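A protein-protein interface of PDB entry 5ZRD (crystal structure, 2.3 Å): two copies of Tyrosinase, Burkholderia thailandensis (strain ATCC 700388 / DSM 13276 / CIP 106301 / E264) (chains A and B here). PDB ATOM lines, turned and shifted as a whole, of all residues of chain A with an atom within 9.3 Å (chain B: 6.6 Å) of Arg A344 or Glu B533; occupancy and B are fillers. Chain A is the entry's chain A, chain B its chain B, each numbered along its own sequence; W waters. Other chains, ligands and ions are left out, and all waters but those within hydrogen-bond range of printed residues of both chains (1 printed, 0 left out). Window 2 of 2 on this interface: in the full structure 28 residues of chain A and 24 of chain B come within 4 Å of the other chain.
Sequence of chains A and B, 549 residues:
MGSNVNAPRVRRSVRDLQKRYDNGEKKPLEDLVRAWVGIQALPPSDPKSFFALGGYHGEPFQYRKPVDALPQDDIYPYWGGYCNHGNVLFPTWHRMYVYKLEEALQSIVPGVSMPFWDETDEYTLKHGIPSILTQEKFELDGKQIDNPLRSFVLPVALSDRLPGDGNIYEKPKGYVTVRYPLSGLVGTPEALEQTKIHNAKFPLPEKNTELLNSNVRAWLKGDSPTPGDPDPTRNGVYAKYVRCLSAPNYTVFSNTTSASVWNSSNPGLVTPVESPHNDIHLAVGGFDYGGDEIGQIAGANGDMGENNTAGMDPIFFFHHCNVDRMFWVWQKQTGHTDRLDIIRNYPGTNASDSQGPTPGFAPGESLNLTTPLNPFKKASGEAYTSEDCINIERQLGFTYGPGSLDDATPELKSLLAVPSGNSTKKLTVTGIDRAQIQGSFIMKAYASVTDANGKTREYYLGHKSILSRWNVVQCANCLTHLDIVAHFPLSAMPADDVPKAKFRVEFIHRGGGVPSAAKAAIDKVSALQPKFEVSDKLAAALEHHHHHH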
ATOM      1  N   VAL A  88      -6.399 -16.453   7.024  1.00  0.00           N
ATOM      2  CA  VAL A  88      -5.136 -15.707   6.771  1.00  0.00           C
ATOM      3  C   VAL A  88      -5.142 -14.326   7.447  1.00  0.00           C
ATOM      4  O   VAL A  88      -4.107 -13.668   7.521  1.00  0.00           O
ATOM      5  CB  VAL A  88      -4.863 -15.573   5.261  1.00  0.00           C
ATOM      6  CG1 VAL A  88      -4.540 -16.928   4.652  1.00  0.00           C
ATOM      7  CG2 VAL A  88      -6.031 -14.930   4.525  1.00  0.00           C
ATOM      8  N   THR A 251       0.836 -17.472   3.752  1.00  0.00           N
ATOM      9  CA  THR A 251      -0.432 -18.205   3.829  1.00  0.00           C
ATOM     10  C   THR A 251      -0.351 -19.304   4.906  1.00  0.00           C
ATOM     11  O   THR A 251      -1.226 -19.354   5.770  1.00  0.00           O
ATOM     12  CB  THR A 251      -0.879 -18.716   2.458  1.00  0.00           C
ATOM     13  OG1 THR A 251      -0.983 -17.595   1.575  1.00  0.00           O
ATOM     14  CG2 THR A 251      -2.218 -19.414   2.517  1.00  0.00           C
ATOM     15  N   LEU A 340       3.466  -8.933   1.856  1.00  0.00           N
ATOM     16  CA  LEU A 340       2.873 -10.207   2.123  1.00  0.00           C
ATOM     17  C   LEU A 340       2.157 -10.622   0.842  1.00  0.00           C
ATOM     18  O   LEU A 340       1.770  -9.771   0.042  1.00  0.00           O
ATOM     19  CB  LEU A 340       1.895 -10.090   3.302  1.00  0.00           C
ATOM     20  CG  LEU A 340       2.521  -9.763   4.657  1.00  0.00           C
ATOM     21  CD1 LEU A 340       1.441  -9.575   5.711  1.00  0.00           C
ATOM     22  CD2 LEU A 340       3.475 -10.858   5.100  1.00  0.00           C
ATOM     23  N   ASP A 341       1.990 -11.912   0.667  1.00  0.00           N
ATOM     24  CA  ASP A 341       1.133 -12.407  -0.369  1.00  0.00           C
ATOM     25  C   ASP A 341       0.323 -13.540   0.261  1.00  0.00           C
ATOM     26  O   ASP A 341       0.727 -14.143   1.232  1.00  0.00           O
ATOM     27  CB  ASP A 341       1.975 -12.892  -1.556  1.00  0.00           C
ATOM     28  CG  ASP A 341       3.106 -13.825  -1.127  1.00  0.00           C
ATOM     29  OD1 ASP A 341       4.187 -13.340  -0.724  1.00  0.00           O
ATOM     30  OD2 ASP A 341       2.924 -15.043  -1.182  1.00  0.00           O
ATOM     31  N   ILE A 342      -0.823 -13.790  -0.341  1.00  0.00           N
ATOM     32  CA  ILE A 342      -1.764 -14.773   0.034  1.00  0.00           C
ATOM     33  C   ILE A 342      -2.100 -15.582  -1.214  1.00  0.00           C
ATOM     34  O   ILE A 342      -2.315 -15.017  -2.260  1.00  0.00           O
ATOM     35  CB  ILE A 342      -2.977 -14.047   0.644  1.00  0.00           C
ATOM     36  CG1 ILE A 342      -2.558 -13.445   1.990  1.00  0.00           C
ATOM     37  CG2 ILE A 342      -4.204 -14.949   0.765  1.00  0.00           C
ATOM     38  CD1 ILE A 342      -3.687 -13.000   2.848  1.00  0.00           C
ATOM     39  N   ILE A 343      -2.088 -16.906  -1.120  1.00  0.00           N
ATOM     40  CA  ILE A 343      -2.465 -17.741  -2.262  1.00  0.00           C
ATOM     41  C   ILE A 343      -3.966 -17.651  -2.478  1.00  0.00           C
ATOM     42  O   ILE A 343      -4.720 -18.098  -1.629  1.00  0.00           O
ATOM     43  CB  ILE A 343      -2.045 -19.190  -2.009  1.00  0.00           C
ATOM     44  CG1 ILE A 343      -0.521 -19.306  -1.980  1.00  0.00           C
ATOM     45  CG2 ILE A 343      -2.696 -20.128  -3.007  1.00  0.00           C
ATOM     46  CD1 ILE A 343      -0.028 -20.491  -1.171  1.00  0.00           C
ATOM     47  N   ARG A 344      -4.387 -17.095  -3.606  1.00  0.00           N
ATOM     48  CA  ARG A 344      -5.812 -16.893  -3.869  1.00  0.00           C
ATOM     49  C   ARG A 344      -6.553 -18.237  -3.765  1.00  0.00           C
ATOM     50  O   ARG A 344      -6.198 -19.217  -4.387  1.00  0.00           O
ATOM     51  CB  ARG A 344      -6.034 -16.250  -5.247  1.00  0.00           C
ATOM     52  CG  ARG A 344      -6.482 -14.792  -5.216  1.00  0.00           C
ATOM     53  CD  ARG A 344      -5.369 -13.794  -4.886  1.00  0.00           C
ATOM     54  NE  ARG A 344      -4.503 -13.422  -6.016  1.00  0.00           N
ATOM     55  CZ  ARG A 344      -4.141 -12.173  -6.345  1.00  0.00           C
ATOM     56  NH1 ARG A 344      -3.259 -11.969  -7.314  1.00  0.00           N
ATOM     57  NH2 ARG A 344      -4.653 -11.135  -5.704  1.00  0.00           N
ATOM     58  N   ASN A 345      -7.571 -18.260  -2.945  1.00  0.00           N
ATOM     59  CA  ASN A 345      -8.558 -19.341  -2.863  1.00  0.00           C
ATOM     60  C   ASN A 345      -7.983 -20.584  -2.182  1.00  0.00           C
ATOM     61  O   ASN A 345      -8.625 -21.655  -2.263  1.00  0.00           O
ATOM     62  CB  ASN A 345      -9.171 -19.680  -4.221  1.00  0.00           C
ATOM     63  CG  ASN A 345     -10.160 -18.624  -4.697  1.00  0.00           C
ATOM     64  OD1 ASN A 345     -11.000 -18.187  -3.934  1.00  0.00           O
ATOM     65  ND2 ASN A 345     -10.106 -18.239  -5.963  1.00  0.00           N
ATOM     66  N   TYR A 346      -6.817 -20.450  -1.541  1.00  0.00           N
ATOM     67  CA  TYR A 346      -6.277 -21.499  -0.706  1.00  0.00           C
ATOM     68  C   TYR A 346      -7.146 -21.646   0.551  1.00  0.00           C
ATOM     69  O   TYR A 346      -7.639 -20.681   1.069  1.00  0.00           O
ATOM     70  CB  TYR A 346      -4.826 -21.217  -0.311  1.00  0.00           C
ATOM     71  CG  TYR A 346      -4.004 -22.445   0.003  1.00  0.00           C
ATOM     72  CD1 TYR A 346      -3.523 -23.244  -1.007  1.00  0.00           C
ATOM     73  CD2 TYR A 346      -3.647 -22.787   1.308  1.00  0.00           C
ATOM     74  CE1 TYR A 346      -2.716 -24.344  -0.751  1.00  0.00           C
ATOM     75  CE2 TYR A 346      -2.882 -23.915   1.588  1.00  0.00           C
ATOM     76  CZ  TYR A 346      -2.425 -24.707   0.542  1.00  0.00           C
ATOM     77  OH  TYR A 346      -1.626 -25.800   0.746  1.00  0.00           O
ATOM     78  N   PRO A 347      -7.301 -22.867   1.051  1.00  0.00           N
ATOM     79  CA  PRO A 347      -8.035 -23.014   2.301  1.00  0.00           C
ATOM     80  C   PRO A 347      -7.430 -22.075   3.345  1.00  0.00           C
ATOM     81  O   PRO A 347      -6.205 -21.996   3.452  1.00  0.00           O
ATOM     82  CB  PRO A 347      -7.871 -24.496   2.664  1.00  0.00           C
ATOM     83  CG  PRO A 347      -7.842 -25.136   1.313  1.00  0.00           C
ATOM     84  CD  PRO A 347      -6.935 -24.191   0.541  1.00  0.00           C
ATOM     85  N   GLY A 348      -8.291 -21.388   4.089  1.00  0.00           N
ATOM     86  CA  GLY A 348      -7.852 -20.305   4.994  1.00  0.00           C
ATOM     87  C   GLY A 348      -8.146 -18.921   4.414  1.00  0.00           C
ATOM     88  O   GLY A 348      -8.061 -17.957   5.129  1.00  0.00           O
ATOM     89  N   THR A 349      -8.508 -18.825   3.139  1.00  0.00           N
ATOM     90  CA  THR A 349      -8.768 -17.511   2.509  1.00  0.00           C
ATOM     91  C   THR A 349     -10.263 -17.309   2.299  1.00  0.00           C
ATOM     92  O   THR A 349     -10.632 -16.391   1.578  1.00  0.00           O
ATOM     93  CB  THR A 349      -8.085 -17.336   1.148  1.00  0.00           C
ATOM     94  OG1 THR A 349      -8.560 -18.346   0.272  1.00  0.00           O
ATOM     95  CG2 THR A 349      -6.585 -17.434   1.207  1.00  0.00           C
ATOM     96  N   ASN A 350     -11.093 -18.134   2.942  1.00  0.00           N
ATOM     97  CA  ASN A 350     -12.520 -17.964   2.863  1.00  0.00           C
ATOM     98  C   ASN A 350     -13.178 -17.626   4.221  1.00  0.00           C
ATOM     99  O   ASN A 350     -12.870 -18.161   5.305  1.00  0.00           O
ATOM    100  CB  ASN A 350     -13.193 -19.190   2.275  1.00  0.00           C
ATOM    101  CG  ASN A 350     -14.408 -18.728   1.499  1.00  0.00           C
ATOM    102  OD1 ASN A 350     -14.288 -18.255   0.365  1.00  0.00           O
ATOM    103  ND2 ASN A 350     -15.560 -18.741   2.137  1.00  0.00           N
ATOM    104  N   SER A 366     -14.375 -13.987  -0.047  1.00  0.00           N
ATOM    105  CA  SER A 366     -12.930 -14.089  -0.062  1.00  0.00           C
ATOM    106  C   SER A 366     -12.322 -13.137   0.970  1.00  0.00           C
ATOM    107  O   SER A 366     -12.739 -11.990   1.088  1.00  0.00           O
ATOM    108  CB  SER A 366     -12.372 -13.836  -1.448  1.00  0.00           C
ATOM    109  OG  SER A 366     -11.114 -13.189  -1.358  1.00  0.00           O
ATOM    110  N   LEU A 367     -11.320 -13.646   1.693  1.00  0.00           N
ATOM    111  CA  LEU A 367     -10.480 -12.877   2.568  1.00  0.00           C
ATOM    112  C   LEU A 367      -9.122 -12.676   1.894  1.00  0.00           C
ATOM    113  O   LEU A 367      -8.519 -13.652   1.390  1.00  0.00           O
ATOM    114  CB  LEU A 367     -10.291 -13.620   3.894  1.00  0.00           C
ATOM    115  CG  LEU A 367     -11.567 -14.096   4.570  1.00  0.00           C
ATOM    116  CD1 LEU A 367     -11.267 -14.851   5.866  1.00  0.00           C
ATOM    117  CD2 LEU A 367     -12.466 -12.917   4.858  1.00  0.00           C
ATOM    118  N   ASN A 368      -8.636 -11.432   1.937  1.00  0.00           N
ATOM    119  CA  ASN A 368      -7.362 -11.060   1.316  1.00  0.00           C
ATOM    120  C   ASN A 368      -6.759  -9.837   2.050  1.00  0.00           C
ATOM    121  O   ASN A 368      -7.220  -9.468   3.140  1.00  0.00           O
ATOM    122  CB  ASN A 368      -7.598 -10.847  -0.178  1.00  0.00           C
ATOM    123  CG  ASN A 368      -8.603  -9.740  -0.400  1.00  0.00           C
ATOM    124  OD1 ASN A 368      -8.350  -8.610   0.006  1.00  0.00           O
ATOM    125  ND2 ASN A 368      -9.771 -10.082  -0.923  1.00  0.00           N
ATOM    126  N   LEU A 369      -5.725  -9.210   1.493  1.00  0.00           N
ATOM    127  CA  LEU A 369      -4.976  -8.140   2.230  1.00  0.00           C
ATOM    128  C   LEU A 369      -5.760  -6.825   2.237  1.00  0.00           C
ATOM    129  O   LEU A 369      -5.398  -5.889   2.955  1.00  0.00           O
ATOM    130  CB  LEU A 369      -3.602  -7.931   1.588  1.00  0.00           C
ATOM    131  CG  LEU A 369      -2.682  -9.151   1.638  1.00  0.00           C
ATOM    132  CD1 LEU A 369      -1.605  -9.069   0.569  1.00  0.00           C
ATOM    133  CD2 LEU A 369      -2.070  -9.315   3.014  1.00  0.00           C
ATOM    134  N   THR A 370      -6.832  -6.804   1.447  1.00  0.00           N
ATOM    135  CA  THR A 370      -7.776  -5.696   1.259  1.00  0.00           C
ATOM    136  C   THR A 370      -8.936  -5.800   2.254  1.00  0.00           C
ATOM    137  O   THR A 370      -9.667  -4.846   2.447  1.00  0.00           O
ATOM    138  CB  THR A 370      -8.240  -5.721  -0.214  1.00  0.00           C
ATOM    139  OG1 THR A 370      -7.296  -4.869  -0.847  1.00  0.00           O
ATOM    140  CG2 THR A 370      -9.644  -5.246  -0.512  1.00  0.00           C
ATOM    141  N   GLU A 387      -3.183  -4.332   4.658  1.00  0.00           N
ATOM    142  CA  GLU A 387      -2.193  -3.592   3.828  1.00  0.00           C
ATOM    143  C   GLU A 387      -1.637  -2.429   4.658  1.00  0.00           C
ATOM    144  O   GLU A 387      -0.508  -2.050   4.484  1.00  0.00           O
ATOM    145  CB  GLU A 387      -2.813  -3.200   2.478  1.00  0.00           C
ATOM    146  CG  GLU A 387      -1.804  -3.003   1.351  1.00  0.00           C
ATOM    147  CD  GLU A 387      -1.412  -4.203   0.486  1.00  0.00           C
ATOM    148  OE1 GLU A 387      -2.321  -4.805  -0.131  1.00  0.00           O
ATOM    149  OE2 GLU A 387      -0.183  -4.502   0.381  1.00  0.00           O
ATOM    150  N   SER B 260      -7.668 -24.428 -10.373  1.00  0.00           N
ATOM    151  CA  SER B 260      -7.483 -23.001 -10.244  1.00  0.00           C
ATOM    152  C   SER B 260      -6.513 -22.719  -9.092  1.00  0.00           C
ATOM    153  O   SER B 260      -5.564 -21.964  -9.252  1.00  0.00           O
ATOM    154  CB  SER B 260      -8.809 -22.284 -10.045  1.00  0.00           C
ATOM    155  OG  SER B 260      -8.579 -20.890  -9.896  1.00  0.00           O
ATOM    156  N   VAL B 261      -6.795 -23.302  -7.938  1.00  0.00           N
ATOM    157  CA  VAL B 261      -5.954 -23.116  -6.800  1.00  0.00           C
ATOM    158  C   VAL B 261      -4.558 -23.696  -7.098  1.00  0.00           C
ATOM    159  O   VAL B 261      -3.529 -23.075  -6.762  1.00  0.00           O
ATOM    160  CB  VAL B 261      -6.568 -23.716  -5.517  1.00  0.00           C
ATOM    161  CG1 VAL B 261      -5.611 -23.610  -4.340  1.00  0.00           C
ATOM    162  CG2 VAL B 261      -7.836 -22.978  -5.156  1.00  0.00           C
ATOM    163  N   SER B 264      -2.661 -21.222  -8.942  1.00  0.00           N
ATOM    164  CA  SER B 264      -2.202 -20.069  -8.102  1.00  0.00           C
ATOM    165  C   SER B 264      -1.021 -20.441  -7.190  1.00  0.00           C
ATOM    166  O   SER B 264      -0.485 -19.567  -6.567  1.00  0.00           O
ATOM    167  CB  SER B 264      -3.327 -19.527  -7.257  1.00  0.00           C
ATOM    168  OG  SER B 264      -4.371 -18.961  -8.052  1.00  0.00           O
ATOM    169  N   LYS B 426       2.782 -16.733 -16.818  1.00  0.00           N
ATOM    170  CA  LYS B 426       1.366 -16.782 -16.887  1.00  0.00           C
ATOM    171  C   LYS B 426       0.787 -15.551 -16.183  1.00  0.00           C
ATOM    172  O   LYS B 426       1.395 -14.960 -15.286  1.00  0.00           O
ATOM    173  CB  LYS B 426       0.889 -18.123 -16.324  1.00  0.00           C
ATOM    174  CG  LYS B 426       0.946 -18.229 -14.819  1.00  0.00           C
ATOM    175  CD  LYS B 426       0.685 -19.651 -14.288  1.00  0.00           C
ATOM    176  CE  LYS B 426       0.767 -19.697 -12.785  1.00  0.00           C
ATOM    177  NZ  LYS B 426       1.087 -21.061 -12.330  1.00  0.00           N
ATOM    178  N   LEU B 427      -0.389 -15.190 -16.665  1.00  0.00           N
ATOM    179  CA  LEU B 427      -1.114 -14.036 -16.202  1.00  0.00           C
ATOM    180  C   LEU B 427      -2.220 -14.481 -15.245  1.00  0.00           C
ATOM    181  O   LEU B 427      -2.981 -15.410 -15.548  1.00  0.00           O
ATOM    182  CB  LEU B 427      -1.738 -13.374 -17.429  1.00  0.00           C
ATOM    183  CG  LEU B 427      -2.589 -12.160 -17.141  1.00  0.00           C
ATOM    184  CD1 LEU B 427      -1.704 -10.986 -16.816  1.00  0.00           C
ATOM    185  CD2 LEU B 427      -3.498 -11.817 -18.324  1.00  0.00           C
ATOM    186  N   THR B 428      -2.353 -13.782 -14.125  1.00  0.00           N
ATOM    187  CA  THR B 428      -3.431 -14.048 -13.187  1.00  0.00           C
ATOM    188  C   THR B 428      -4.382 -12.859 -13.159  1.00  0.00           C
ATOM    189  O   THR B 428      -3.967 -11.731 -12.889  1.00  0.00           O
ATOM    190  CB  THR B 428      -2.902 -14.361 -11.785  1.00  0.00           C
ATOM    191  OG1 THR B 428      -1.929 -15.405 -11.869  1.00  0.00           O
ATOM    192  CG2 THR B 428      -4.011 -14.793 -10.855  1.00  0.00           C
ATOM    193  N   VAL B 429      -5.646 -13.141 -13.463  1.00  0.00           N
ATOM    194  CA  VAL B 429      -6.697 -12.126 -13.476  1.00  0.00           C
ATOM    195  C   VAL B 429      -7.622 -12.323 -12.273  1.00  0.00           C
ATOM    196  O   VAL B 429      -8.267 -13.396 -12.116  1.00  0.00           O
ATOM    197  CB  VAL B 429      -7.525 -12.186 -14.763  1.00  0.00           C
ATOM    198  CG1 VAL B 429      -8.546 -11.077 -14.764  1.00  0.00           C
ATOM    199  CG2 VAL B 429      -6.675 -12.137 -16.017  1.00  0.00           C
ATOM    200  N   THR B 430      -7.690 -11.290 -11.450  1.00  0.00           N
ATOM    201  CA  THR B 430      -8.559 -11.286 -10.289  1.00  0.00           C
ATOM    202  C   THR B 430      -9.378 -10.000 -10.288  1.00  0.00           C
ATOM    203  O   THR B 430      -8.939  -8.973 -10.714  1.00  0.00           O
ATOM    204  CB  THR B 430      -7.787 -11.487  -8.992  1.00  0.00           C
ATOM    205  OG1 THR B 430      -6.933 -10.370  -8.768  1.00  0.00           O
ATOM    206  CG2 THR B 430      -6.970 -12.756  -9.059  1.00  0.00           C
ATOM    207  N   ASP B 483     -16.427 -14.541  -6.787  1.00  0.00           N
ATOM    208  CA  ASP B 483     -14.973 -14.313  -6.792  1.00  0.00           C
ATOM    209  C   ASP B 483     -14.278 -14.826  -8.097  1.00  0.00           C
ATOM    210  O   ASP B 483     -14.044 -16.036  -8.279  1.00  0.00           O
ATOM    211  CB  ASP B 483     -14.379 -15.003  -5.549  1.00  0.00           C
ATOM    212  CG  ASP B 483     -12.869 -15.197  -5.635  1.00  0.00           C
ATOM    213  OD1 ASP B 483     -12.113 -14.223  -5.403  1.00  0.00           O
ATOM    214  OD2 ASP B 483     -12.451 -16.337  -5.927  1.00  0.00           O
ATOM    215  N   VAL B 485     -11.458 -15.734 -10.474  1.00  0.00           N
ATOM    216  CA  VAL B 485     -10.004 -16.005 -10.595  1.00  0.00           C
ATOM    217  C   VAL B 485      -9.715 -16.759 -11.899  1.00  0.00           C
ATOM    218  O   VAL B 485     -10.296 -17.797 -12.126  1.00  0.00           O
ATOM    219  CB  VAL B 485      -9.444 -16.765  -9.382  1.00  0.00           C
ATOM    220  CG1 VAL B 485     -10.182 -18.087  -9.173  1.00  0.00           C
ATOM    221  CG2 VAL B 485      -7.945 -17.000  -9.528  1.00  0.00           C
ATOM    222  N   LEU B 490       1.108 -16.826 -21.286  1.00  0.00           N
ATOM    223  CA  LEU B 490       1.706 -15.691 -22.014  1.00  0.00           C
ATOM    224  C   LEU B 490       2.598 -16.218 -23.150  1.00  0.00           C
ATOM    225  O   LEU B 490       3.307 -15.458 -23.769  1.00  0.00           O
ATOM    226  CB  LEU B 490       2.470 -14.779 -21.039  1.00  0.00           C
ATOM    227  CG  LEU B 490       1.568 -14.037 -20.041  1.00  0.00           C
ATOM    228  CD1 LEU B 490       2.326 -13.490 -18.837  1.00  0.00           C
ATOM    229  CD2 LEU B 490       0.812 -12.918 -20.735  1.00  0.00           C
ATOM    230  N   PHE B 503      -2.942  -5.240 -20.212  1.00  0.00           N
ATOM    231  CA  PHE B 503      -3.810  -6.396 -20.274  1.00  0.00           C
ATOM    232  C   PHE B 503      -5.265  -5.959 -20.230  1.00  0.00           C
ATOM    233  O   PHE B 503      -5.533  -4.951 -19.627  1.00  0.00           O
ATOM    234  CB  PHE B 503      -3.524  -7.323 -19.094  1.00  0.00           C
ATOM    235  CG  PHE B 503      -2.169  -7.963 -19.174  1.00  0.00           C
ATOM    236  CD1 PHE B 503      -1.934  -8.965 -20.088  1.00  0.00           C
ATOM    237  CD2 PHE B 503      -1.131  -7.523 -18.364  1.00  0.00           C
ATOM    238  CE1 PHE B 503      -0.695  -9.573 -20.143  1.00  0.00           C
ATOM    239  CE2 PHE B 503       0.117  -8.109 -18.441  1.00  0.00           C
ATOM    240  CZ  PHE B 503       0.319  -9.150 -19.312  1.00  0.00           C
ATOM    241  N   LYS B 531      -7.850  -6.827 -11.687  1.00  0.00           N
ATOM    242  CA  LYS B 531      -6.439  -6.767 -11.330  1.00  0.00           C
ATOM    243  C   LYS B 531      -5.680  -7.826 -12.159  1.00  0.00           C
ATOM    244  O   LYS B 531      -6.213  -8.907 -12.477  1.00  0.00           O
ATOM    245  CB  LYS B 531      -6.307  -6.938  -9.814  1.00  0.00           C
ATOM    246  CG  LYS B 531      -4.956  -6.554  -9.217  1.00  0.00           C
ATOM    247  CD  LYS B 531      -3.980  -7.718  -9.079  1.00  0.00           C
ATOM    248  CE  LYS B 531      -2.590  -7.309  -8.626  1.00  0.00           C
ATOM    249  NZ  LYS B 531      -2.615  -6.635  -7.306  1.00  0.00           N
ATOM    250  N   PHE B 532      -4.446  -7.499 -12.545  1.00  0.00           N
ATOM    251  CA  PHE B 532      -3.598  -8.378 -13.364  1.00  0.00           C
ATOM    252  C   PHE B 532      -2.245  -8.608 -12.685  1.00  0.00           C
ATOM    253  O   PHE B 532      -1.610  -7.670 -12.208  1.00  0.00           O
ATOM    254  CB  PHE B 532      -3.363  -7.778 -14.752  1.00  0.00           C
ATOM    255  CG  PHE B 532      -4.618  -7.571 -15.558  1.00  0.00           C
ATOM    256  CD1 PHE B 532      -5.191  -8.628 -16.249  1.00  0.00           C
ATOM    257  CD2 PHE B 532      -5.226  -6.327 -15.616  1.00  0.00           C
ATOM    258  CE1 PHE B 532      -6.348  -8.445 -16.981  1.00  0.00           C
ATOM    259  CE2 PHE B 532      -6.374  -6.141 -16.366  1.00  0.00           C
ATOM    260  CZ  PHE B 532      -6.938  -7.202 -17.034  1.00  0.00           C
ATOM    261  N   GLU B 533      -1.811  -9.862 -12.672  1.00  0.00           N
ATOM    262  CA  GLU B 533      -0.569 -10.232 -12.054  1.00  0.00           C
ATOM    263  C   GLU B 533       0.194 -11.165 -13.001  1.00  0.00           C
ATOM    264  O   GLU B 533      -0.384 -12.038 -13.636  1.00  0.00           O
ATOM    265  CB  GLU B 533      -0.915 -10.860 -10.710  1.00  0.00           C
ATOM    266  CG  GLU B 533       0.257 -11.184  -9.818  1.00  0.00           C
ATOM    267  CD  GLU B 533      -0.219 -11.665  -8.457  1.00  0.00           C
ATOM    268  OE1 GLU B 533       0.306 -12.701  -7.983  1.00  0.00           O
ATOM    269  OE2 GLU B 533      -1.148 -11.015  -7.891  1.00  0.00           O
ATOM    270  N   VAL B 534       1.494 -10.946 -13.095  1.00  0.00           N
ATOM    271  CA  VAL B 534       2.389 -11.756 -13.867  1.00  0.00           C
ATOM    272  C   VAL B 534       3.285 -12.569 -12.930  1.00  0.00           C
ATOM    273  O   VAL B 534       3.801 -12.034 -11.977  1.00  0.00           O
ATOM    274  CB  VAL B 534       3.257 -10.879 -14.778  1.00  0.00           C
ATOM    275  CG1 VAL B 534       4.196 -11.748 -15.601  1.00  0.00           C
ATOM    276  CG2 VAL B 534       2.376  -9.986 -15.637  1.00  0.00           C
ATOM    277  N   SER B 535       3.504 -13.841 -13.281  1.00  0.00           N
ATOM    278  CA  SER B 535       4.289 -14.781 -12.469  1.00  0.00           C
ATOM    279  C   SER B 535       5.791 -14.699 -12.807  1.00  0.00           C
ATOM    280  O   SER B 535       6.235 -13.815 -13.567  1.00  0.00           O
ATOM    281  CB  SER B 535       3.765 -16.192 -12.663  1.00  0.00           C
ATOM    282  OG  SER B 535       4.196 -16.729 -13.900  1.00  0.00           O
HETATM  283  O   HOH W   1      -6.718 -19.364  -7.102  1.00  0.00           O
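Water W1 bridges OG of Ser B264 (2.6 Å) and O of Arg A344 (2.8 Å).
Val B534 touches none of the printed residues of chain A.
Printed residues of chain B within 4 Å of Tyr A346: Val B261.
Of the printed residues of chain A, Val B261 touches Asn A345 and Tyr A346.
Printed residues of chain A within 4 Å of Val B485: Asn A345 (3.2 Å).
Of the printed residues of chain B, Ser A366 touches Asp B483 (3.98 Å).
Ile A342 touches none of the printed residues of chain B.
The nearest residue of chain B that does not touch Arg A344 is Ser B264 (4.1 Å).
OD2 of Asp B483 sits at hydrogen-bond distance from ND2 of Asn A345.
The guanidinium group (NH1) of Arg A344 lies within salt-bridge range of the side-chain carboxylate (OE1) of Glu B533 (3.7 Å).
Among the printed residues, merely in contact across the chains: Asn A345 with Val B485 (3.2 Å), Asn A345 with Val B261 (3.3 Å), Arg A344 with Thr B430 (3.9 Å), Tyr A346 with Val B261 (3.95 Å) and Ser A366 with Asp B483 (3.98 Å).
No position is printed for both chains.
Of the 7 pairs that touch across the chains among the printed residues, none has its exchanged pair printed and touching as well.
O of Tyr A346 sits at hydrogen-bond distance from OG1 of Thr A349, at 2.6 Å.
The backbone carbonyl oxygen (O) of Glu B533 sits at hydrogen-bond distance from the backbone NH (N) of Thr B428 (2.7 Å).
The backbone NH (N) of Lys B531 sits at hydrogen-bond distance from the backbone carbonyl oxygen (O) of Thr B430.
The side-chain hydroxyl (OG) of Ser A366 sits at hydrogen-bond distance from the side-chain amide nitrogen (ND2) of Asn A368 (3.4 Å).
The backbone NH (N) of Asn A345 sits close to the side-chain hydroxyl (OG1) of Thr A349 (3.4 Å).
Hydrophobic or aromatic side chains of chain A within 4 Å of the printed part of chain B: Tyr A346.
Printed residues of chain B that touch a printed residue of chain A: Val B261, Thr B430, Asp B483, Val B485 and Glu B533.
Among the printed residues, Asp or Glu carboxylates within 4 Å of a Lys or Arg side-chain nitrogen of the other chain: Arg A344 with Glu B533 (2.4 Å).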
